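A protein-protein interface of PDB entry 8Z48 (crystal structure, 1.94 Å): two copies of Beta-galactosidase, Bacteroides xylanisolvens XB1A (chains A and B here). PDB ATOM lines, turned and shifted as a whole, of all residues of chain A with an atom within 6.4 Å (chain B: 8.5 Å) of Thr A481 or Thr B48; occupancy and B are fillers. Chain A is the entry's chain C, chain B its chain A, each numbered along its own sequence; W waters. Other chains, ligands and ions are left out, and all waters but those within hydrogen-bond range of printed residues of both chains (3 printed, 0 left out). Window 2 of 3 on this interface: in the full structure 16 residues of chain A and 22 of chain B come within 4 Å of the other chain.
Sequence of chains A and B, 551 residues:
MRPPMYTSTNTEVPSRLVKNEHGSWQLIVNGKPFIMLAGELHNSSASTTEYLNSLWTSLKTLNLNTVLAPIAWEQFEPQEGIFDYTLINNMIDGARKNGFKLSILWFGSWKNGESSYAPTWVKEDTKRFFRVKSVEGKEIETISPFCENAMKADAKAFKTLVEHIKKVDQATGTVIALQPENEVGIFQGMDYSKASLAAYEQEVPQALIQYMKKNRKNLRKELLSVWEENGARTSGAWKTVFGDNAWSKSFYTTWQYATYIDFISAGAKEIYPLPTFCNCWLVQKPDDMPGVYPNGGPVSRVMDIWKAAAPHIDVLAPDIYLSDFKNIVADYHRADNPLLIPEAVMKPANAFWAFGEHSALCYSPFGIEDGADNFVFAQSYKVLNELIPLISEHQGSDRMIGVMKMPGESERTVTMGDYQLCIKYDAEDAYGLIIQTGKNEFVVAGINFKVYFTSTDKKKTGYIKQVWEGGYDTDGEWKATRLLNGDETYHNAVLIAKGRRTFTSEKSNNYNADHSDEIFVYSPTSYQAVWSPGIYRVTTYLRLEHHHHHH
Of chain A, only Thr A481 comes within 4 Å of Thr B48.
Ala A480 touches none of the printed residues of chain B.
Printed residues of chain A within 4 Å of Glu B50: Lys A479 (2.6 Å).
Of the printed residues of chain A, Tyr B51 touches Thr A481 (3.5 Å) and Arg A482 (3.5 Å).
Ala B46 touches none of the printed residues of chain A.
Gly A471 touches none of the printed residues of chain B.
The nearest residue of chain B that does not touch Thr A481 is Ser B47 (4.7 Å).
The side-chain hydroxyl of Ser B47 sits at hydrogen-bond distance from the backbone carbonyl oxygen of Ser B44.
O of Gly A471 is in hydrogen-bond range of N of Lys A479.
The backbone carbonyl oxygen (O) of Ser B47 lies within hydrogen-bond range of the side-chain amide nitrogen (NE2) of Gln B75 (3.0 Å).
OG1 of Thr B49 lies within hydrogen-bond range of OE1 of Glu B50 (3.2 Å).
The side-chain hydroxyl (OG1) of Thr B48 lies within hydrogen-bond range of the backbone NH (N) of Tyr B51, 3.1 Å away.
The guanidinium group (NE) of Arg A482 lies within salt-bridge range of the side-chain carboxylate (OE1) of Glu A469, at 3.1 Å.
Thr A481 touches Tyr B51 (O to CB, 3.5 Å).
Arg A482 touches Ser B44.
Ser B47 touches Arg A482.
Tyr B51 touches Arg A482 (CE2 to CD, 3.5 Å).
Ser B44 touches Leu A483.
CG of Gln B75 touches CD1 of Leu A483, at 3.96 Å.
Water W1 lies within hydrogen-bond range of the side-chain carboxylate (OE1) of Glu B50 (2.5 Å) and the side-chain amino group (NZ) of Lys A479 (3.2 Å).
Water W3 bridges the guanidinium group (NH1) of Arg A482 (2.7 Å) and the side-chain hydroxyl (OG) of Ser B45 (3.0 Å).
Water W2 bridges the backbone carbonyl oxygen of Ala A480 and the side-chain carboxylate of Glu B50.
No position is printed for both chains.
Of the 9 pairs that touch across the chains among the printed residues, none has its exchanged pair printed and touching as well.
Hydrophobic or aromatic side chains of chain B within 4 Å of the printed part of chain A: Tyr B51.
Of the 10 printed residues of chain A, 4 touch a printed residue of chain B.
Hydrophobic or aromatic side chains of chain A within 4 Å of the printed part of chain B: Leu A483.
Among the printed residues, 9 pairs touch across the chains.
Among the printed residues, Asp or Glu carboxylates within 4 Å of a Lys or Arg side-chain nitrogen of the other chain: Lys A479 with Glu B50.
NZ of Lys A479 lies within salt-bridge range of OE2 of Glu B50.
O of Thr A481 lies within hydrogen-bond range of OG1 of Thr B48 (2.7 Å).
The backbone NH of Leu A483 lies within hydrogen-bond range of the side-chain hydroxyl of Ser B47, at 2.9 Å.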
ATOM      1  N   TRP A 468     -25.116  28.578 -34.690  1.00  0.00           N
ATOM      2  CA  TRP A 468     -24.868  27.408 -33.868  1.00  0.00           C
ATOM      3  C   TRP A 468     -23.380  27.047 -33.957  1.00  0.00           C
ATOM      4  O   TRP A 468     -22.757  27.131 -35.016  1.00  0.00           O
ATOM      5  CB  TRP A 468     -25.723  26.203 -34.289  1.00  0.00           C
ATOM      6  CG  TRP A 468     -27.219  26.400 -34.333  1.00  0.00           C
ATOM      7  CD1 TRP A 468     -28.159  26.021 -33.411  1.00  0.00           C
ATOM      8  CD2 TRP A 468     -27.943  26.976 -35.433  1.00  0.00           C
ATOM      9  NE1 TRP A 468     -29.418  26.343 -33.855  1.00  0.00           N
ATOM     10  CE2 TRP A 468     -29.316  26.936 -35.090  1.00  0.00           C
ATOM     11  CE3 TRP A 468     -27.562  27.517 -36.670  1.00  0.00           C
ATOM     12  CZ2 TRP A 468     -30.292  27.416 -35.958  1.00  0.00           C
ATOM     13  CZ3 TRP A 468     -28.531  28.000 -37.520  1.00  0.00           C
ATOM     14  CH2 TRP A 468     -29.882  27.954 -37.160  1.00  0.00           C
ATOM     15  N   GLU A 469     -22.815  26.718 -32.800  1.00  0.00           N
ATOM     16  CA  GLU A 469     -21.523  26.088 -32.703  1.00  0.00           C
ATOM     17  C   GLU A 469     -21.771  24.591 -32.665  1.00  0.00           C
ATOM     18  O   GLU A 469     -22.723  24.147 -32.038  1.00  0.00           O
ATOM     19  CB  GLU A 469     -20.844  26.518 -31.412  1.00  0.00           C
ATOM     20  CG  GLU A 469     -19.667  25.656 -30.961  1.00  0.00           C
ATOM     21  CD  GLU A 469     -19.262  26.131 -29.587  1.00  0.00           C
ATOM     22  OE1 GLU A 469     -19.619  25.534 -28.512  1.00  0.00           O
ATOM     23  OE2 GLU A 469     -18.609  27.184 -29.644  1.00  0.00           O
ATOM     24  N   GLY A 470     -20.879  23.821 -33.294  1.00  0.00           N
ATOM     25  CA  GLY A 470     -20.961  22.384 -33.166  1.00  0.00           C
ATOM     26  C   GLY A 470     -19.860  21.680 -33.945  1.00  0.00           C
ATOM     27  O   GLY A 470     -18.757  22.197 -34.100  1.00  0.00           O
ATOM     28  N   GLY A 471     -20.213  20.479 -34.409  1.00  0.00           N
ATOM     29  CA  GLY A 471     -19.278  19.595 -35.059  1.00  0.00           C
ATOM     30  C   GLY A 471     -20.044  18.471 -35.732  1.00  0.00           C
ATOM     31  O   GLY A 471     -21.272  18.423 -35.595  1.00  0.00           O
ATOM     32  N   TRP A 478     -24.245  16.561 -38.431  1.00  0.00           N
ATOM     33  CA  TRP A 478     -24.063  17.776 -37.647  1.00  0.00           C
ATOM     34  C   TRP A 478     -24.772  17.667 -36.301  1.00  0.00           C
ATOM     35  O   TRP A 478     -25.891  17.195 -36.219  1.00  0.00           O
ATOM     36  CB  TRP A 478     -24.603  18.973 -38.431  1.00  0.00           C
ATOM     37  CG  TRP A 478     -24.654  20.261 -37.659  1.00  0.00           C
ATOM     38  CD1 TRP A 478     -25.765  20.852 -37.140  1.00  0.00           C
ATOM     39  CD2 TRP A 478     -23.547  21.137 -37.357  1.00  0.00           C
ATOM     40  NE1 TRP A 478     -25.428  22.026 -36.530  1.00  0.00           N
ATOM     41  CE2 TRP A 478     -24.079  22.237 -36.654  1.00  0.00           C
ATOM     42  CE3 TRP A 478     -22.168  21.090 -37.586  1.00  0.00           C
ATOM     43  CZ2 TRP A 478     -23.278  23.279 -36.190  1.00  0.00           C
ATOM     44  CZ3 TRP A 478     -21.375  22.124 -37.133  1.00  0.00           C
ATOM     45  CH2 TRP A 478     -21.927  23.202 -36.441  1.00  0.00           C
ATOM     46  N   LYS A 479     -24.082  18.097 -35.247  1.00  0.00           N
ATOM     47  CA  LYS A 479     -24.649  18.205 -33.914  1.00  0.00           C
ATOM     48  C   LYS A 479     -24.210  19.547 -33.323  1.00  0.00           C
ATOM     49  O   LYS A 479     -23.022  19.756 -33.071  1.00  0.00           O
ATOM     50  CB  LYS A 479     -24.124  16.964 -33.187  1.00  0.00           C
ATOM     51  CG  LYS A 479     -24.448  16.783 -31.729  1.00  0.00           C
ATOM     52  CD  LYS A 479     -25.927  16.955 -31.387  1.00  0.00           C
ATOM     53  CE  LYS A 479     -26.257  15.960 -30.337  1.00  0.00           C
ATOM     54  NZ  LYS A 479     -27.209  16.451 -29.354  1.00  0.00           N
ATOM     55  N   ALA A 480     -25.176  20.430 -33.063  1.00  0.00           N
ATOM     56  CA  ALA A 480     -24.892  21.687 -32.399  1.00  0.00           C
ATOM     57  C   ALA A 480     -24.648  21.420 -30.912  1.00  0.00           C
ATOM     58  O   ALA A 480     -25.304  20.564 -30.305  1.00  0.00           O
ATOM     59  CB  ALA A 480     -26.027  22.652 -32.658  1.00  0.00           C
ATOM     60  N   THR A 481     -23.652  22.120 -30.363  1.00  0.00           N
ATOM     61  CA  THR A 481     -23.334  22.120 -28.941  1.00  0.00           C
ATOM     62  C   THR A 481     -23.967  23.358 -28.279  1.00  0.00           C
ATOM     63  O   THR A 481     -24.333  23.325 -27.106  1.00  0.00           O
ATOM     64  CB  THR A 481     -21.813  22.059 -28.718  1.00  0.00           C
ATOM     65  OG1 THR A 481     -21.126  23.033 -29.501  1.00  0.00           O
ATOM     66  CG2 THR A 481     -21.191  20.705 -29.044  1.00  0.00           C
ATOM     67  N   ARG A 482     -24.086  24.462 -29.025  1.00  0.00           N
ATOM     68  CA  ARG A 482     -24.762  25.652 -28.521  1.00  0.00           C
ATOM     69  C   ARG A 482     -25.421  26.355 -29.701  1.00  0.00           C
ATOM     70  O   ARG A 482     -24.937  26.275 -30.823  1.00  0.00           O
ATOM     71  CB  ARG A 482     -23.822  26.596 -27.767  1.00  0.00           C
ATOM     72  CG  ARG A 482     -23.318  26.134 -26.407  1.00  0.00           C
ATOM     73  CD  ARG A 482     -22.386  27.148 -25.706  1.00  0.00           C
ATOM     74  NE  ARG A 482     -21.042  27.236 -26.298  1.00  0.00           N
ATOM     75  CZ  ARG A 482     -20.189  28.220 -26.095  1.00  0.00           C
ATOM     76  NH1 ARG A 482     -20.497  29.196 -25.264  1.00  0.00           N
ATOM     77  NH2 ARG A 482     -19.013  28.209 -26.690  1.00  0.00           N
ATOM     78  N   LEU A 483     -26.558  26.985 -29.438  1.00  0.00           N
ATOM     79  CA  LEU A 483     -27.005  28.114 -30.231  1.00  0.00           C
ATOM     80  C   LEU A 483     -26.283  29.311 -29.619  1.00  0.00           C
ATOM     81  O   LEU A 483     -26.429  29.562 -28.439  1.00  0.00           O
ATOM     82  CB  LEU A 483     -28.536  28.239 -30.218  1.00  0.00           C
ATOM     83  CG  LEU A 483     -29.142  29.134 -31.309  1.00  0.00           C
ATOM     84  CD1 LEU A 483     -30.609  28.856 -31.476  1.00  0.00           C
ATOM     85  CD2 LEU A 483     -28.903  30.647 -31.014  1.00  0.00           C
ATOM     86  N   LEU B  41     -25.859  31.914 -15.617  1.00  0.00           N
ATOM     87  CA  LEU B  41     -25.090  31.293 -16.675  1.00  0.00           C
ATOM     88  C   LEU B  41     -24.833  32.338 -17.757  1.00  0.00           C
ATOM     89  O   LEU B  41     -25.593  33.295 -17.931  1.00  0.00           O
ATOM     90  CB  LEU B  41     -25.868  30.101 -17.238  1.00  0.00           C
ATOM     91  CG  LEU B  41     -26.341  29.037 -16.251  1.00  0.00           C
ATOM     92  CD1 LEU B  41     -26.962  27.874 -17.028  1.00  0.00           C
ATOM     93  CD2 LEU B  41     -25.242  28.566 -15.326  1.00  0.00           C
ATOM     94  N   ASN B  43     -24.923  33.586 -21.542  1.00  0.00           N
ATOM     95  CA  ASN B  43     -26.137  33.708 -22.329  1.00  0.00           C
ATOM     96  C   ASN B  43     -26.435  32.416 -23.097  1.00  0.00           C
ATOM     97  O   ASN B  43     -27.606  32.052 -23.205  1.00  0.00           O
ATOM     98  CB  ASN B  43     -26.023  34.884 -23.291  1.00  0.00           C
ATOM     99  CG  ASN B  43     -25.977  36.254 -22.657  1.00  0.00           C
ATOM    100  OD1 ASN B  43     -25.521  37.192 -23.323  1.00  0.00           O
ATOM    101  ND2 ASN B  43     -26.488  36.426 -21.438  1.00  0.00           N
ATOM    102  N   SER B  44     -25.412  31.793 -23.731  1.00  0.00           N
ATOM    103  CA  SER B  44     -25.599  30.659 -24.633  1.00  0.00           C
ATOM    104  C   SER B  44     -25.464  29.278 -23.937  1.00  0.00           C
ATOM    105  O   SER B  44     -25.572  28.218 -24.577  1.00  0.00           O
ATOM    106  CB  SER B  44     -24.672  30.753 -25.832  1.00  0.00           C
ATOM    107  OG  SER B  44     -24.773  31.995 -26.539  1.00  0.00           O
ATOM    108  N   SER B  45     -25.301  29.249 -22.610  1.00  0.00           N
ATOM    109  CA  SER B  45     -25.018  28.024 -21.876  1.00  0.00           C
ATOM    110  C   SER B  45     -26.232  27.123 -21.660  1.00  0.00           C
ATOM    111  O   SER B  45     -26.031  25.964 -21.288  1.00  0.00           O
ATOM    112  CB  SER B  45     -24.389  28.274 -20.539  1.00  0.00           C
ATOM    113  OG  SER B  45     -23.203  29.032 -20.659  1.00  0.00           O
ATOM    114  N   ALA B  46     -27.463  27.630 -21.843  1.00  0.00           N
ATOM    115  CA  ALA B  46     -28.639  26.794 -21.682  1.00  0.00           C
ATOM    116  C   ALA B  46     -29.283  26.533 -23.055  1.00  0.00           C
ATOM    117  O   ALA B  46     -30.432  26.116 -23.115  1.00  0.00           O
ATOM    118  CB  ALA B  46     -29.593  27.412 -20.678  1.00  0.00           C
ATOM    119  N   SER B  47     -28.536  26.759 -24.144  1.00  0.00           N
ATOM    120  CA  SER B  47     -29.065  26.637 -25.494  1.00  0.00           C
ATOM    121  C   SER B  47     -29.157  25.172 -25.944  1.00  0.00           C
ATOM    122  O   SER B  47     -29.735  24.892 -26.981  1.00  0.00           O
ATOM    123  CB  SER B  47     -28.308  27.456 -26.490  1.00  0.00           C
ATOM    124  OG  SER B  47     -26.918  27.167 -26.552  1.00  0.00           O
ATOM    125  N   THR B  48     -28.540  24.241 -25.215  1.00  0.00           N
ATOM    126  CA  THR B  48     -28.720  22.820 -25.493  1.00  0.00           C
ATOM    127  C   THR B  48     -28.800  22.082 -24.169  1.00  0.00           C
ATOM    128  O   THR B  48     -28.304  22.599 -23.157  1.00  0.00           O
ATOM    129  CB  THR B  48     -27.604  22.198 -26.340  1.00  0.00           C
ATOM    130  OG1 THR B  48     -26.361  22.365 -25.654  1.00  0.00           O
ATOM    131  CG2 THR B  48     -27.570  22.720 -27.764  1.00  0.00           C
ATOM    132  N   THR B  49     -29.330  20.842 -24.210  1.00  0.00           N
ATOM    133  CA  THR B  49     -29.359  20.011 -23.020  1.00  0.00           C
ATOM    134  C   THR B  49     -27.948  19.578 -22.656  1.00  0.00           C
ATOM    135  O   THR B  49     -27.583  19.594 -21.480  1.00  0.00           O
ATOM    136  CB  THR B  49     -30.265  18.786 -23.189  1.00  0.00           C
ATOM    137  OG1 THR B  49     -29.664  17.933 -24.155  1.00  0.00           O
ATOM    138  CG2 THR B  49     -31.670  19.146 -23.615  1.00  0.00           C
ATOM    139  N   GLU B  50     -27.139  19.193 -23.655  1.00  0.00           N
ATOM    140  CA  GLU B  50     -25.822  18.666 -23.346  1.00  0.00           C
ATOM    141  C   GLU B  50     -24.946  19.753 -22.695  1.00  0.00           C
ATOM    142  O   GLU B  50     -24.188  19.469 -21.766  1.00  0.00           O
ATOM    143  CB  GLU B  50     -25.172  18.016 -24.568  1.00  0.00           C
ATOM    144  CG  GLU B  50     -25.956  16.840 -25.141  1.00  0.00           C
ATOM    145  CD  GLU B  50     -27.023  17.215 -26.153  1.00  0.00           C
ATOM    146  OE1 GLU B  50     -27.332  18.428 -26.330  1.00  0.00           O
ATOM    147  OE2 GLU B  50     -27.528  16.253 -26.782  1.00  0.00           O
ATOM    148  N   TYR B  51     -25.010  20.998 -23.181  1.00  0.00           N
ATOM    149  CA  TYR B  51     -24.076  22.016 -22.700  1.00  0.00           C
ATOM    150  C   TYR B  51     -24.440  22.410 -21.272  1.00  0.00           C
ATOM    151  O   TYR B  51     -23.583  22.458 -20.392  1.00  0.00           O
ATOM    152  CB  TYR B  51     -24.021  23.255 -23.593  1.00  0.00           C
ATOM    153  CG  TYR B  51     -22.867  24.190 -23.243  1.00  0.00           C
ATOM    154  CD1 TYR B  51     -22.993  25.169 -22.250  1.00  0.00           C
ATOM    155  CD2 TYR B  51     -21.647  24.083 -23.895  1.00  0.00           C
ATOM    156  CE1 TYR B  51     -21.941  26.008 -21.926  1.00  0.00           C
ATOM    157  CE2 TYR B  51     -20.601  24.940 -23.603  1.00  0.00           C
ATOM    158  CZ  TYR B  51     -20.741  25.893 -22.607  1.00  0.00           C
ATOM    159  OH  TYR B  51     -19.674  26.718 -22.374  1.00  0.00           O
ATOM    160  N   LEU B  52     -25.733  22.642 -21.021  1.00  0.00           N
ATOM    161  CA  LEU B  52     -26.166  22.907 -19.652  1.00  0.00           C
ATOM    162  C   LEU B  52     -25.741  21.754 -18.747  1.00  0.00           C
ATOM    163  O   LEU B  52     -25.273  21.978 -17.636  1.00  0.00           O
ATOM    164  CB  LEU B  52     -27.666  23.158 -19.538  1.00  0.00           C
ATOM    165  CG  LEU B  52     -28.210  23.374 -18.117  1.00  0.00           C
ATOM    166  CD1 LEU B  52     -27.595  24.570 -17.439  1.00  0.00           C
ATOM    167  CD2 LEU B  52     -29.700  23.540 -18.147  1.00  0.00           C
ATOM    168  N   ASN B  53     -25.957  20.507 -19.190  1.00  0.00           N
ATOM    169  CA  ASN B  53     -25.809  19.379 -18.274  1.00  0.00           C
ATOM    170  C   ASN B  53     -24.347  19.234 -17.858  1.00  0.00           C
ATOM    171  O   ASN B  53     -24.071  18.802 -16.742  1.00  0.00           O
ATOM    172  CB  ASN B  53     -26.404  18.087 -18.824  1.00  0.00           C
ATOM    173  CG  ASN B  53     -27.911  18.093 -18.786  1.00  0.00           C
ATOM    174  OD1 ASN B  53     -28.534  18.939 -18.142  1.00  0.00           O
ATOM    175  ND2 ASN B  53     -28.525  17.137 -19.452  1.00  0.00           N
ATOM    176  N   SER B  54     -23.434  19.705 -18.714  1.00  0.00           N
ATOM    177  CA  SER B  54     -22.016  19.662 -18.419  1.00  0.00           C
ATOM    178  C   SER B  54     -21.634  20.613 -17.291  1.00  0.00           C
ATOM    179  O   SER B  54     -20.550  20.458 -16.765  1.00  0.00           O
ATOM    180  CB  SER B  54     -21.195  19.944 -19.644  1.00  0.00           C
ATOM    181  OG  SER B  54     -21.256  21.326 -19.990  1.00  0.00           O
ATOM    182  N   LEU B  55     -22.507  21.549 -16.886  1.00  0.00           N
ATOM    183  CA  LEU B  55     -22.164  22.595 -15.918  1.00  0.00           C
ATOM    184  C   LEU B  55     -22.506  22.288 -14.448  1.00  0.00           C
ATOM    185  O   LEU B  55     -21.882  22.868 -13.551  1.00  0.00           O
ATOM    186  CB  LEU B  55     -22.881  23.871 -16.364  1.00  0.00           C
ATOM    187  CG  LEU B  55     -22.568  24.345 -17.788  1.00  0.00           C
ATOM    188  CD1 LEU B  55     -23.267  25.682 -18.057  1.00  0.00           C
ATOM    189  CD2 LEU B  55     -21.031  24.424 -18.040  1.00  0.00           C
ATOM    190  N   TRP B  56     -23.474  21.398 -14.173  1.00  0.00           N
ATOM    191  CA  TRP B  56     -24.122  21.360 -12.866  1.00  0.00           C
ATOM    192  C   TRP B  56     -23.127  21.020 -11.746  1.00  0.00           C
ATOM    193  O   TRP B  56     -23.286  21.509 -10.625  1.00  0.00           O
ATOM    194  CB  TRP B  56     -25.275  20.359 -12.832  1.00  0.00           C
ATOM    195  CG  TRP B  56     -26.415  20.543 -13.796  1.00  0.00           C
ATOM    196  CD1 TRP B  56     -26.734  19.698 -14.822  1.00  0.00           C
ATOM    197  CD2 TRP B  56     -27.463  21.526 -13.753  1.00  0.00           C
ATOM    198  NE1 TRP B  56     -27.865  20.125 -15.452  1.00  0.00           N
ATOM    199  CE2 TRP B  56     -28.347  21.231 -14.810  1.00  0.00           C
ATOM    200  CE3 TRP B  56     -27.732  22.632 -12.955  1.00  0.00           C
ATOM    201  CZ2 TRP B  56     -29.482  21.993 -15.073  1.00  0.00           C
ATOM    202  CZ3 TRP B  56     -28.849  23.388 -13.215  1.00  0.00           C
ATOM    203  CH2 TRP B  56     -29.727  23.065 -14.250  1.00  0.00           C
ATOM    204  N   PRO B  70     -31.549  31.372 -18.944  1.00  0.00           N
ATOM    205  CA  PRO B  70     -32.549  31.790 -19.929  1.00  0.00           C
ATOM    206  C   PRO B  70     -33.265  30.646 -20.640  1.00  0.00           C
ATOM    207  O   PRO B  70     -32.683  29.591 -20.879  1.00  0.00           O
ATOM    208  CB  PRO B  70     -31.719  32.576 -20.928  1.00  0.00           C
ATOM    209  CG  PRO B  70     -30.427  31.808 -20.952  1.00  0.00           C
ATOM    210  CD  PRO B  70     -30.196  31.386 -19.494  1.00  0.00           C
ATOM    211  N   GLN B  75     -36.049  29.505 -29.555  1.00  0.00           N
ATOM    212  CA  GLN B  75     -36.021  28.053 -29.416  1.00  0.00           C
ATOM    213  C   GLN B  75     -37.317  27.493 -28.845  1.00  0.00           C
ATOM    214  O   GLN B  75     -37.695  26.355 -29.149  1.00  0.00           O
ATOM    215  CB  GLN B  75     -34.909  27.614 -28.466  1.00  0.00           C
ATOM    216  CG  GLN B  75     -33.537  28.072 -28.927  1.00  0.00           C
ATOM    217  CD  GLN B  75     -32.501  27.700 -27.916  1.00  0.00           C
ATOM    218  OE1 GLN B  75     -32.492  28.269 -26.817  1.00  0.00           O
ATOM    219  NE2 GLN B  75     -31.726  26.673 -28.260  1.00  0.00           N
ATOM    220  N   THR B  86     -38.259  20.991 -24.536  1.00  0.00           N
ATOM    221  CA  THR B  86     -37.053  20.242 -24.222  1.00  0.00           C
ATOM    222  C   THR B  86     -36.162  20.998 -23.229  1.00  0.00           C
ATOM    223  O   THR B  86     -35.689  20.407 -22.257  1.00  0.00           O
ATOM    224  CB  THR B  86     -36.273  19.950 -25.506  1.00  0.00           C
ATOM    225  OG1 THR B  86     -37.145  19.259 -26.395  1.00  0.00           O
ATOM    226  CG2 THR B  86     -35.062  19.074 -25.238  1.00  0.00           C
ATOM    227  N   LEU B  87     -35.886  22.284 -23.500  1.00  0.00           N
ATOM    228  CA  LEU B  87     -34.877  23.011 -22.742  1.00  0.00           C
ATOM    229  C   LEU B  87     -35.414  23.315 -21.346  1.00  0.00           C
ATOM    230  O   LEU B  87     -34.748  23.035 -20.350  1.00  0.00           O
ATOM    231  CB  LEU B  87     -34.356  24.228 -23.517  1.00  0.00           C
ATOM    232  CG  LEU B  87     -33.610  23.891 -24.819  1.00  0.00           C
ATOM    233  CD1 LEU B  87     -33.193  25.127 -25.626  1.00  0.00           C
ATOM    234  CD2 LEU B  87     -32.368  23.046 -24.593  1.00  0.00           C
ATOM    235  N   ASN B  90     -35.503  19.878 -19.238  1.00  0.00           N
ATOM    236  CA  ASN B  90     -34.201  19.379 -18.839  1.00  0.00           C
ATOM    237  C   ASN B  90     -33.591  20.313 -17.791  1.00  0.00           C
ATOM    238  O   ASN B  90     -32.918  19.863 -16.853  1.00  0.00           O
ATOM    239  CB  ASN B  90     -33.269  19.231 -20.029  1.00  0.00           C
ATOM    240  CG  ASN B  90     -31.845  18.943 -19.602  1.00  0.00           C
ATOM    241  OD1 ASN B  90     -31.500  17.782 -19.337  1.00  0.00           O
ATOM    242  ND2 ASN B  90     -31.003  19.958 -19.527  1.00  0.00           N
ATOM    243  N   MET B  91     -33.846  21.615 -17.942  1.00  0.00           N
ATOM    244  CA  MET B  91     -33.345  22.579 -16.967  1.00  0.00           C
ATOM    245  C   MET B  91     -33.911  22.268 -15.579  1.00  0.00           C
ATOM    246  O   MET B  91     -33.168  22.166 -14.610  1.00  0.00           O
ATOM    247  CB  MET B  91     -33.653  24.004 -17.430  1.00  0.00           C
ATOM    248  CG  MET B  91     -33.272  25.088 -16.431  1.00  0.00           C
ATOM    249  SD  MET B  91     -33.608  26.731 -17.107  1.00  0.00           S
ATOM    250  CE  MET B  91     -32.707  26.764 -18.662  1.00  0.00           C
HETATM  251  O   HOH W   1     -29.018  18.763 -28.113  1.00  0.00           O
HETATM  252  O   HOH W   2     -25.091  19.132 -27.954  1.00  0.00           O
HETATM  253  O   HOH W   3     -22.234  30.057 -23.320  1.00  0.00           O
